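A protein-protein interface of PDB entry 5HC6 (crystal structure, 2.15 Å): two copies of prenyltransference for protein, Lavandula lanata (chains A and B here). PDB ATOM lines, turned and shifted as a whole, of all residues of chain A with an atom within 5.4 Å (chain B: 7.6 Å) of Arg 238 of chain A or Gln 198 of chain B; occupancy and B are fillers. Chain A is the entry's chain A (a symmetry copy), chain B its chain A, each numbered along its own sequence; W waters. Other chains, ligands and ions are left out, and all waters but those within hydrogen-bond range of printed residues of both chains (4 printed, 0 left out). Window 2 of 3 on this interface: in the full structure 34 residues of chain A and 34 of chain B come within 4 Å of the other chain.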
ATOM      1  N   GLN A 198       3.664 -36.507  16.116  1.00  0.00           N
ATOM      2  CA  GLN A 198       2.378 -35.983  16.594  1.00  0.00           C
ATOM      3  C   GLN A 198       1.709 -37.019  17.471  1.00  0.00           C
ATOM      4  O   GLN A 198       0.792 -37.728  17.025  1.00  0.00           O
ATOM      5  CB  GLN A 198       1.475 -35.574  15.412  1.00  0.00           C
ATOM      6  CG  GLN A 198       1.988 -34.323  14.628  1.00  0.00           C
ATOM      7  CD  GLN A 198       1.205 -34.033  13.365  1.00  0.00           C
ATOM      8  OE1 GLN A 198       1.647 -34.339  12.277  1.00  0.00           O
ATOM      9  NE2 GLN A 198      -0.001 -33.609  13.520  1.00  0.00           N
ATOM     10  N   THR A 211      -5.778 -28.418  26.351  1.00  0.00           N
ATOM     11  CA  THR A 211      -4.537 -27.818  25.966  1.00  0.00           C
ATOM     12  C   THR A 211      -4.343 -27.734  24.427  1.00  0.00           C
ATOM     13  O   THR A 211      -4.731 -28.603  23.663  1.00  0.00           O
ATOM     14  CB  THR A 211      -3.326 -28.458  26.656  1.00  0.00           C
ATOM     15  OG1 THR A 211      -2.507 -29.141  25.737  1.00  0.00           O
ATOM     16  CG2 THR A 211      -3.678 -29.288  27.793  1.00  0.00           C
ATOM     17  N   GLU A 212      -3.787 -26.627  23.980  1.00  0.00           N
ATOM     18  CA  GLU A 212      -3.428 -26.477  22.571  1.00  0.00           C
ATOM     19  C   GLU A 212      -2.128 -27.208  22.319  1.00  0.00           C
ATOM     20  O   GLU A 212      -1.138 -27.030  23.052  1.00  0.00           O
ATOM     21  CB  GLU A 212      -3.233 -24.998  22.226  1.00  0.00           C
ATOM     22  CG  GLU A 212      -4.509 -24.148  22.378  1.00  0.00           C
ATOM     23  CD  GLU A 212      -5.543 -24.441  21.299  1.00  0.00           C
ATOM     24  OE1 GLU A 212      -5.143 -24.900  20.226  1.00  0.00           O
ATOM     25  OE2 GLU A 212      -6.747 -24.241  21.516  1.00  0.00           O
ATOM     26  N   PHE A 213      -2.105 -27.992  21.257  1.00  0.00           N
ATOM     27  CA  PHE A 213      -0.907 -28.637  20.841  1.00  0.00           C
ATOM     28  C   PHE A 213      -0.156 -27.845  19.768  1.00  0.00           C
ATOM     29  O   PHE A 213      -0.774 -27.312  18.901  1.00  0.00           O
ATOM     30  CB  PHE A 213      -1.278 -29.985  20.278  1.00  0.00           C
ATOM     31  CG  PHE A 213      -1.959 -30.908  21.256  1.00  0.00           C
ATOM     32  CD1 PHE A 213      -1.710 -30.844  22.591  1.00  0.00           C
ATOM     33  CD2 PHE A 213      -2.885 -31.807  20.809  1.00  0.00           C
ATOM     34  CE1 PHE A 213      -2.311 -31.733  23.465  1.00  0.00           C
ATOM     35  CE2 PHE A 213      -3.504 -32.686  21.666  1.00  0.00           C
ATOM     36  CZ  PHE A 213      -3.213 -32.664  22.999  1.00  0.00           C
ATOM     37  N   TYR A 214       1.179 -27.811  19.838  1.00  0.00           N
ATOM     38  CA  TYR A 214       2.026 -27.194  18.831  1.00  0.00           C
ATOM     39  C   TYR A 214       3.156 -28.142  18.523  1.00  0.00           C
ATOM     40  O   TYR A 214       3.946 -28.479  19.402  1.00  0.00           O
ATOM     41  CB  TYR A 214       2.597 -25.892  19.369  1.00  0.00           C
ATOM     42  CG  TYR A 214       3.589 -25.169  18.468  1.00  0.00           C
ATOM     43  CD1 TYR A 214       3.160 -24.350  17.421  1.00  0.00           C
ATOM     44  CD2 TYR A 214       4.938 -25.329  18.657  1.00  0.00           C
ATOM     45  CE1 TYR A 214       4.083 -23.690  16.610  1.00  0.00           C
ATOM     46  CE2 TYR A 214       5.863 -24.712  17.847  1.00  0.00           C
ATOM     47  CZ  TYR A 214       5.435 -23.866  16.848  1.00  0.00           C
ATOM     48  OH  TYR A 214       6.387 -23.258  16.070  1.00  0.00           O
ATOM     49  N   PHE A 215       3.230 -28.556  17.266  1.00  0.00           N
ATOM     50  CA  PHE A 215       4.232 -29.511  16.767  1.00  0.00           C
ATOM     51  C   PHE A 215       5.206 -28.775  15.858  1.00  0.00           C
ATOM     52  O   PHE A 215       4.735 -28.075  15.000  1.00  0.00           O
ATOM     53  CB  PHE A 215       3.494 -30.607  15.995  1.00  0.00           C
ATOM     54  CG  PHE A 215       2.517 -31.363  16.860  1.00  0.00           C
ATOM     55  CD1 PHE A 215       2.955 -32.271  17.797  1.00  0.00           C
ATOM     56  CD2 PHE A 215       1.146 -31.104  16.778  1.00  0.00           C
ATOM     57  CE1 PHE A 215       2.053 -32.923  18.621  1.00  0.00           C
ATOM     58  CE2 PHE A 215       0.244 -31.780  17.585  1.00  0.00           C
ATOM     59  CZ  PHE A 215       0.693 -32.677  18.516  1.00  0.00           C
ATOM     60  N   SER A 234       1.812 -18.852  17.652  1.00  0.00           N
ATOM     61  CA  SER A 234       0.760 -19.821  17.295  1.00  0.00           C
ATOM     62  C   SER A 234      -0.349 -19.815  18.338  1.00  0.00           C
ATOM     63  O   SER A 234      -1.554 -19.755  18.004  1.00  0.00           O
ATOM     64  CB  SER A 234       1.318 -21.236  17.144  1.00  0.00           C
ATOM     65  OG  SER A 234       0.294 -22.166  16.756  1.00  0.00           O
ATOM     66  N   TYR A 235       0.014 -19.863  19.607  1.00  0.00           N
ATOM     67  CA  TYR A 235      -1.019 -19.971  20.649  1.00  0.00           C
ATOM     68  C   TYR A 235      -1.920 -18.733  20.630  1.00  0.00           C
ATOM     69  O   TYR A 235      -3.134 -18.839  20.768  1.00  0.00           O
ATOM     70  CB  TYR A 235      -0.389 -20.170  22.031  1.00  0.00           C
ATOM     71  CG  TYR A 235      -1.334 -20.148  23.230  1.00  0.00           C
ATOM     72  CD1 TYR A 235      -1.995 -21.296  23.641  1.00  0.00           C
ATOM     73  CD2 TYR A 235      -1.544 -18.967  23.965  1.00  0.00           C
ATOM     74  CE1 TYR A 235      -2.856 -21.284  24.721  1.00  0.00           C
ATOM     75  CE2 TYR A 235      -2.415 -18.931  25.063  1.00  0.00           C
ATOM     76  CZ  TYR A 235      -3.063 -20.106  25.424  1.00  0.00           C
ATOM     77  OH  TYR A 235      -3.875 -20.130  26.514  1.00  0.00           O
ATOM     78  N   ARG A 236      -1.328 -17.567  20.426  1.00  0.00           N
ATOM     79  CA  ARG A 236      -2.096 -16.333  20.422  1.00  0.00           C
ATOM     80  C   ARG A 236      -3.052 -16.267  19.232  1.00  0.00           C
ATOM     81  O   ARG A 236      -4.193 -15.849  19.398  1.00  0.00           O
ATOM     82  CB  ARG A 236      -1.175 -15.119  20.508  1.00  0.00           C
ATOM     83  CG  ARG A 236      -0.283 -15.127  21.749  1.00  0.00           C
ATOM     84  CD  ARG A 236       0.316 -13.753  22.057  1.00  0.00           C
ATOM     85  NE  ARG A 236       1.713 -13.791  22.521  1.00  0.00           N
ATOM     86  CZ  ARG A 236       2.795 -13.593  21.755  1.00  0.00           C
ATOM     87  NH1 ARG A 236       2.694 -13.329  20.455  1.00  0.00           N
ATOM     88  NH2 ARG A 236       4.007 -13.651  22.295  1.00  0.00           N
ATOM     89  N   CYS A 237      -2.636 -16.731  18.059  1.00  0.00           N
ATOM     90  CA  CYS A 237      -3.553 -16.866  16.933  1.00  0.00           C
ATOM     91  C   CYS A 237      -4.742 -17.834  17.090  1.00  0.00           C
ATOM     92  O   CYS A 237      -5.614 -17.849  16.242  1.00  0.00           O
ATOM     93  CB  CYS A 237      -2.771 -17.276  15.702  1.00  0.00           C
ATOM     94  SG  CYS A 237      -1.696 -15.936  15.265  1.00  0.00           S
ATOM     95  N   ARG A 238      -4.824 -18.637  18.136  1.00  0.00           N
ATOM     96  CA  ARG A 238      -5.916 -19.621  18.197  1.00  0.00           C
ATOM     97  C   ARG A 238      -7.195 -19.178  18.923  1.00  0.00           C
ATOM     98  O   ARG A 238      -7.168 -18.218  19.695  1.00  0.00           O
ATOM     99  CB  ARG A 238      -5.369 -20.936  18.742  1.00  0.00           C
ATOM    100  CG  ARG A 238      -4.290 -21.499  17.829  1.00  0.00           C
ATOM    101  CD  ARG A 238      -3.763 -22.771  18.386  1.00  0.00           C
ATOM    102  NE  ARG A 238      -2.557 -23.264  17.743  1.00  0.00           N
ATOM    103  CZ  ARG A 238      -2.077 -24.484  17.968  1.00  0.00           C
ATOM    104  NH1 ARG A 238      -2.726 -25.319  18.782  1.00  0.00           N
ATOM    105  NH2 ARG A 238      -0.968 -24.889  17.384  1.00  0.00           N
ATOM    106  N   ASP B  21     -15.976 -31.732  13.820  1.00  0.00           N
ATOM    107  CA  ASP B  21     -15.924 -30.337  14.180  1.00  0.00           C
ATOM    108  C   ASP B  21     -16.043 -29.592  12.841  1.00  0.00           C
ATOM    109  O   ASP B  21     -15.841 -30.176  11.787  1.00  0.00           O
ATOM    110  CB  ASP B  21     -14.587 -29.960  14.912  1.00  0.00           C
ATOM    111  CG  ASP B  21     -14.585 -28.509  15.508  1.00  0.00           C
ATOM    112  OD1 ASP B  21     -15.656 -27.818  15.480  1.00  0.00           O
ATOM    113  OD2 ASP B  21     -13.515 -28.033  15.980  1.00  0.00           O
ATOM    114  N   ARG B 193      -8.833 -35.446  13.662  1.00  0.00           N
ATOM    115  CA  ARG B 193      -9.703 -34.346  14.103  1.00  0.00           C
ATOM    116  C   ARG B 193      -9.889 -33.381  12.948  1.00  0.00           C
ATOM    117  O   ARG B 193      -8.917 -32.868  12.454  1.00  0.00           O
ATOM    118  CB  ARG B 193      -9.153 -33.622  15.335  1.00  0.00           C
ATOM    119  CG  ARG B 193      -9.963 -32.350  15.647  1.00  0.00           C
ATOM    120  CD  ARG B 193      -9.706 -31.730  17.009  1.00  0.00           C
ATOM    121  NE  ARG B 193     -10.645 -30.626  17.203  1.00  0.00           N
ATOM    122  CZ  ARG B 193     -11.193 -30.274  18.342  1.00  0.00           C
ATOM    123  NH1 ARG B 193     -10.917 -30.926  19.451  1.00  0.00           N
ATOM    124  NH2 ARG B 193     -12.045 -29.249  18.355  1.00  0.00           N
ATOM    125  N   ALA B 194     -11.144 -33.203  12.505  1.00  0.00           N
ATOM    126  CA  ALA B 194     -11.481 -32.292  11.436  1.00  0.00           C
ATOM    127  C   ALA B 194     -11.553 -30.851  11.975  1.00  0.00           C
ATOM    128  O   ALA B 194     -11.682 -30.664  13.174  1.00  0.00           O
ATOM    129  CB  ALA B 194     -12.814 -32.685  10.829  1.00  0.00           C
ATOM    130  N   ALA B 195     -11.397 -29.884  11.065  1.00  0.00           N
ATOM    131  CA  ALA B 195     -11.680 -28.472  11.249  1.00  0.00           C
ATOM    132  C   ALA B 195     -10.492 -27.684  11.741  1.00  0.00           C
ATOM    133  O   ALA B 195     -10.584 -26.512  12.018  1.00  0.00           O
ATOM    134  CB  ALA B 195     -12.926 -28.227  12.121  1.00  0.00           C
ATOM    135  N   GLY B 196      -9.339 -28.280  11.812  1.00  0.00           N
ATOM    136  CA  GLY B 196      -8.197 -27.392  12.053  1.00  0.00           C
ATOM    137  C   GLY B 196      -7.697 -27.258  13.488  1.00  0.00           C
ATOM    138  O   GLY B 196      -6.545 -26.954  13.669  1.00  0.00           O
ATOM    139  N   GLU B 197      -8.527 -27.498  14.508  1.00  0.00           N
ATOM    140  CA  GLU B 197      -8.115 -27.229  15.881  1.00  0.00           C
ATOM    141  C   GLU B 197      -7.177 -28.343  16.300  1.00  0.00           C
ATOM    142  O   GLU B 197      -7.375 -29.495  15.895  1.00  0.00           O
ATOM    143  CB  GLU B 197      -9.306 -27.178  16.828  1.00  0.00           C
ATOM    144  CG  GLU B 197     -10.316 -26.072  16.544  1.00  0.00           C
ATOM    145  CD  GLU B 197      -9.675 -24.695  16.356  1.00  0.00           C
ATOM    146  OE1 GLU B 197     -10.204 -23.954  15.531  1.00  0.00           O
ATOM    147  OE2 GLU B 197      -8.660 -24.324  17.008  1.00  0.00           O
ATOM    148  N   GLN B 198      -6.159 -28.000  17.080  1.00  0.00           N
ATOM    149  CA  GLN B 198      -5.185 -28.993  17.553  1.00  0.00           C
ATOM    150  C   GLN B 198      -5.298 -29.130  19.056  1.00  0.00           C
ATOM    151  O   GLN B 198      -4.482 -28.571  19.806  1.00  0.00           O
ATOM    152  CB  GLN B 198      -3.753 -28.608  17.127  1.00  0.00           C
ATOM    153  CG  GLN B 198      -3.503 -28.714  15.588  1.00  0.00           C
ATOM    154  CD  GLN B 198      -2.161 -28.167  15.151  1.00  0.00           C
ATOM    155  OE1 GLN B 198      -2.076 -27.070  14.637  1.00  0.00           O
ATOM    156  NE2 GLN B 198      -1.121 -28.840  15.502  1.00  0.00           N
ATOM    157  N   ARG B 199      -6.305 -29.874  19.476  1.00  0.00           N
ATOM    158  CA  ARG B 199      -6.527 -30.181  20.858  1.00  0.00           C
ATOM    159  C   ARG B 199      -7.563 -31.279  20.928  1.00  0.00           C
ATOM    160  O   ARG B 199      -8.213 -31.594  19.918  1.00  0.00           O
ATOM    161  CB  ARG B 199      -7.026 -28.931  21.595  1.00  0.00           C
ATOM    162  CG  ARG B 199      -8.345 -28.361  21.084  1.00  0.00           C
ATOM    163  CD  ARG B 199      -8.700 -27.035  21.755  1.00  0.00           C
ATOM    164  NE  ARG B 199      -9.930 -26.523  21.169  1.00  0.00           N
ATOM    165  CZ  ARG B 199     -10.063 -25.464  20.367  1.00  0.00           C
ATOM    166  NH1 ARG B 199      -9.044 -24.691  20.048  1.00  0.00           N
ATOM    167  NH2 ARG B 199     -11.269 -25.173  19.893  1.00  0.00           N
ATOM    168  N   LEU B 200      -7.764 -31.810  22.135  1.00  0.00           N
ATOM    169  CA  LEU B 200      -8.639 -32.951  22.357  1.00  0.00           C
ATOM    170  C   LEU B 200     -10.067 -32.612  22.793  1.00  0.00           C
ATOM    171  O   LEU B 200     -10.973 -33.439  22.639  1.00  0.00           O
ATOM    172  CB  LEU B 200      -8.002 -33.857  23.404  1.00  0.00           C
ATOM    173  CG  LEU B 200      -6.591 -34.347  23.075  1.00  0.00           C
ATOM    174  CD1 LEU B 200      -6.052 -35.115  24.266  1.00  0.00           C
ATOM    175  CD2 LEU B 200      -6.526 -35.182  21.776  1.00  0.00           C
ATOM    176  N   SER B 201     -10.249 -31.419  23.350  1.00  0.00           N
ATOM    177  CA  SER B 201     -11.528 -30.946  23.842  1.00  0.00           C
ATOM    178  C   SER B 201     -12.217 -31.938  24.763  1.00  0.00           C
ATOM    179  O   SER B 201     -13.413 -32.089  24.715  1.00  0.00           O
ATOM    180  CB  SER B 201     -12.470 -30.588  22.684  1.00  0.00           C
ATOM    181  OG  SER B 201     -11.834 -29.753  21.707  1.00  0.00           O
ATOM    182  N   TYR B 214      -3.796 -36.880  13.731  1.00  0.00           N
ATOM    183  CA  TYR B 214      -3.869 -36.336  12.385  1.00  0.00           C
ATOM    184  C   TYR B 214      -4.896 -35.234  12.379  1.00  0.00           C
ATOM    185  O   TYR B 214      -6.068 -35.469  12.662  1.00  0.00           O
ATOM    186  CB  TYR B 214      -4.298 -37.426  11.415  1.00  0.00           C
ATOM    187  CG  TYR B 214      -4.520 -36.993   9.972  1.00  0.00           C
ATOM    188  CD1 TYR B 214      -3.454 -36.856   9.080  1.00  0.00           C
ATOM    189  CD2 TYR B 214      -5.784 -36.705   9.523  1.00  0.00           C
ATOM    190  CE1 TYR B 214      -3.675 -36.465   7.760  1.00  0.00           C
ATOM    191  CE2 TYR B 214      -6.018 -36.287   8.234  1.00  0.00           C
ATOM    192  CZ  TYR B 214      -4.969 -36.202   7.345  1.00  0.00           C
ATOM    193  OH  TYR B 214      -5.244 -35.795   6.065  1.00  0.00           O
ATOM    194  N   PHE B 215      -4.445 -34.034  12.041  1.00  0.00           N
ATOM    195  CA  PHE B 215      -5.274 -32.817  12.011  1.00  0.00           C
ATOM    196  C   PHE B 215      -5.473 -32.391  10.563  1.00  0.00           C
ATOM    197  O   PHE B 215      -4.492 -32.327   9.870  1.00  0.00           O
ATOM    198  CB  PHE B 215      -4.541 -31.729  12.800  1.00  0.00           C
ATOM    199  CG  PHE B 215      -4.323 -32.111  14.242  1.00  0.00           C
ATOM    200  CD1 PHE B 215      -5.364 -32.109  15.141  1.00  0.00           C
ATOM    201  CD2 PHE B 215      -3.069 -32.546  14.681  1.00  0.00           C
ATOM    202  CE1 PHE B 215      -5.164 -32.509  16.452  1.00  0.00           C
ATOM    203  CE2 PHE B 215      -2.867 -32.919  16.001  1.00  0.00           C
ATOM    204  CZ  PHE B 215      -3.913 -32.916  16.884  1.00  0.00           C
ATOM    205  N   THR B 216      -6.722 -32.211  10.097  1.00  0.00           N
ATOM    206  CA  THR B 216      -7.014 -31.673   8.783  1.00  0.00           C
ATOM    207  C   THR B 216      -7.749 -30.377   9.000  1.00  0.00           C
ATOM    208  O   THR B 216      -8.655 -30.361   9.821  1.00  0.00           O
ATOM    209  CB  THR B 216      -8.176 -32.360   7.992  1.00  0.00           C
ATOM    210  OG1 THR B 216      -8.615 -33.593   8.573  1.00  0.00           O
ATOM    211  CG2 THR B 216      -7.914 -32.412   6.543  1.00  0.00           C
HETATM  212  O   HOH W   1      -1.592 -33.961  11.078  1.00  0.00           O
HETATM  213  O   HOH W   2      -6.233 -30.758  24.277  1.00  0.00           O
HETATM  214  O   HOH W   3      -6.295 -25.388  17.791  1.00  0.00           O
HETATM  215  O   HOH W   4       1.319 -27.215  15.361  1.00  0.00           O
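The backbone carbonyl oxygen (O) of Gln 198 of chain B sits at hydrogen-bond distance from the backbone NH (N) of Phe 213 of chain A (2.8 Å).
The guanidinium group (NH1) of Arg 199 of chain B is in salt-bridge range of the side-chain carboxylate (OE2) of Glu 212 of chain A, 2.8 Å away.
OE2 of Glu 197 of chain B is in salt-bridge range of NH1 of Arg 199 of chain B, 3.1 Å away.
The guanidinium group (NH1) of Arg 238 of chain A sits at hydrogen-bond distance from the backbone carbonyl oxygen (O) of Phe 213 of chain A (2.8 Å).
NH1 of Arg 238 of chain A lies within salt-bridge range of OE1 of Glu 212 of chain A (2.8 Å).
The backbone carbonyl oxygen of Arg 199 of chain B sits at hydrogen-bond distance from the guanidinium group of Arg 193 of chain B (2.8 Å).
OG of Ser 234 of chain A sits at hydrogen-bond distance from NH2 of Arg 238 of chain A.
Gln 198 of chain A touches Phe 215 of chain B.
Thr 211 of chain A touches Gln 198 of chain B (O to O, 3.9 Å).
Arg 199 of chain B touches Thr 211 of chain A (CB to O, 3.1 Å).
Gln 198 of chain B touches Glu 212 of chain A.
Phe 213 of chain A touches Arg 199 of chain B (CD2 to CA, 3.99 Å).
Phe 213 of chain A touches Leu 200 of chain B (CZ to CG, 3.8 Å).
Phe 215 of chain A touches Gln 198 of chain B (CD2 to NE2, 3.4 Å).
CE2 of Phe 215 of chain B touches CE2 of Phe 215 of chain A (3.7 Å).
OE1 of Gln 198 of chain B touches NH2 of Arg 238 of chain A (3.7 Å).
Of the printed residues of chain A, Gln 198 of chain B touches Thr 211 (3.9 Å), Glu 212 (3.6 Å), Phe 213 (2.8 Å), Phe 215 (3.4 Å) and Arg 238 (3.7 Å).
Printed residues of chain A within 4 Å of Phe 215 of chain B: Gln 198 and Phe 215.
Printed residues of chain B within 4 Å of Thr 211 of chain A: Gln 198 (3.9 Å) and Arg 199 (3.1 Å).
Of the printed residues of chain A, Arg 199 of chain B touches Thr 211, Glu 212 and Phe 213.
Of the printed residues of chain B, Glu 212 of chain A touches Gln 198 and Arg 199.
Cys 237 of chain A touches none of the printed residues of chain B.
Ser 201 of chain B touches none of the printed residues of chain A.
Printed residues of chain A that touch a printed residue of chain B: Gln 198, Thr 211, Glu 212, Phe 213, Phe 215 and Arg 238.
Hydrophobic or aromatic side chains of chain A within 4 Å of the printed part of chain B: Phe 213 and Phe 215.
Of the 13 printed residues of chain B, 4 touch a printed residue of chain A.
Hydrophobic or aromatic side chains of chain B that line the printed part of chain A: Leu 200 and Phe 215.
Among the printed residues, Asp or Glu carboxylates within 4 Å of a Lys or Arg side-chain nitrogen of the other chain: Glu 212 of chain A with Arg 199 of chain B (2.8 Å).
Gln 198 of chain A touches Phe 215 of chain B, and with the chains exchanged Phe 215 of chain A touches Gln 198 of chain B.
Phe 215 of chain A touches its own counterpart, Phe 215 of chain B.
Of the 11 pairs that touch across the chains among the printed residues, 3 have their exchanged pair printed and touching as well.
Water W2 lies within hydrogen-bond range of the backbone carbonyl oxygen of Thr 211 of chain A (2.7 Å) and the backbone NH of Leu 200 of chain B (2.8 Å).
Water W3 lies within hydrogen-bond range of OE2 of Glu 197 of chain B (2.7 Å), N of Gln 198 of chain B (2.7 Å) and OE1 of Glu 212 of chain A (2.7 Å).
Water W4 lies within hydrogen-bond range of NE2 of Gln 198 of chain B (2.9 Å) and N of Phe 215 of chain A (3.0 Å).
Water W1 lies within hydrogen-bond range of the side-chain amide nitrogen (NE2) of Gln 198 of chain A (2.9 Å) and the backbone NH (N) of Phe 215 of chain B (3.0 Å).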
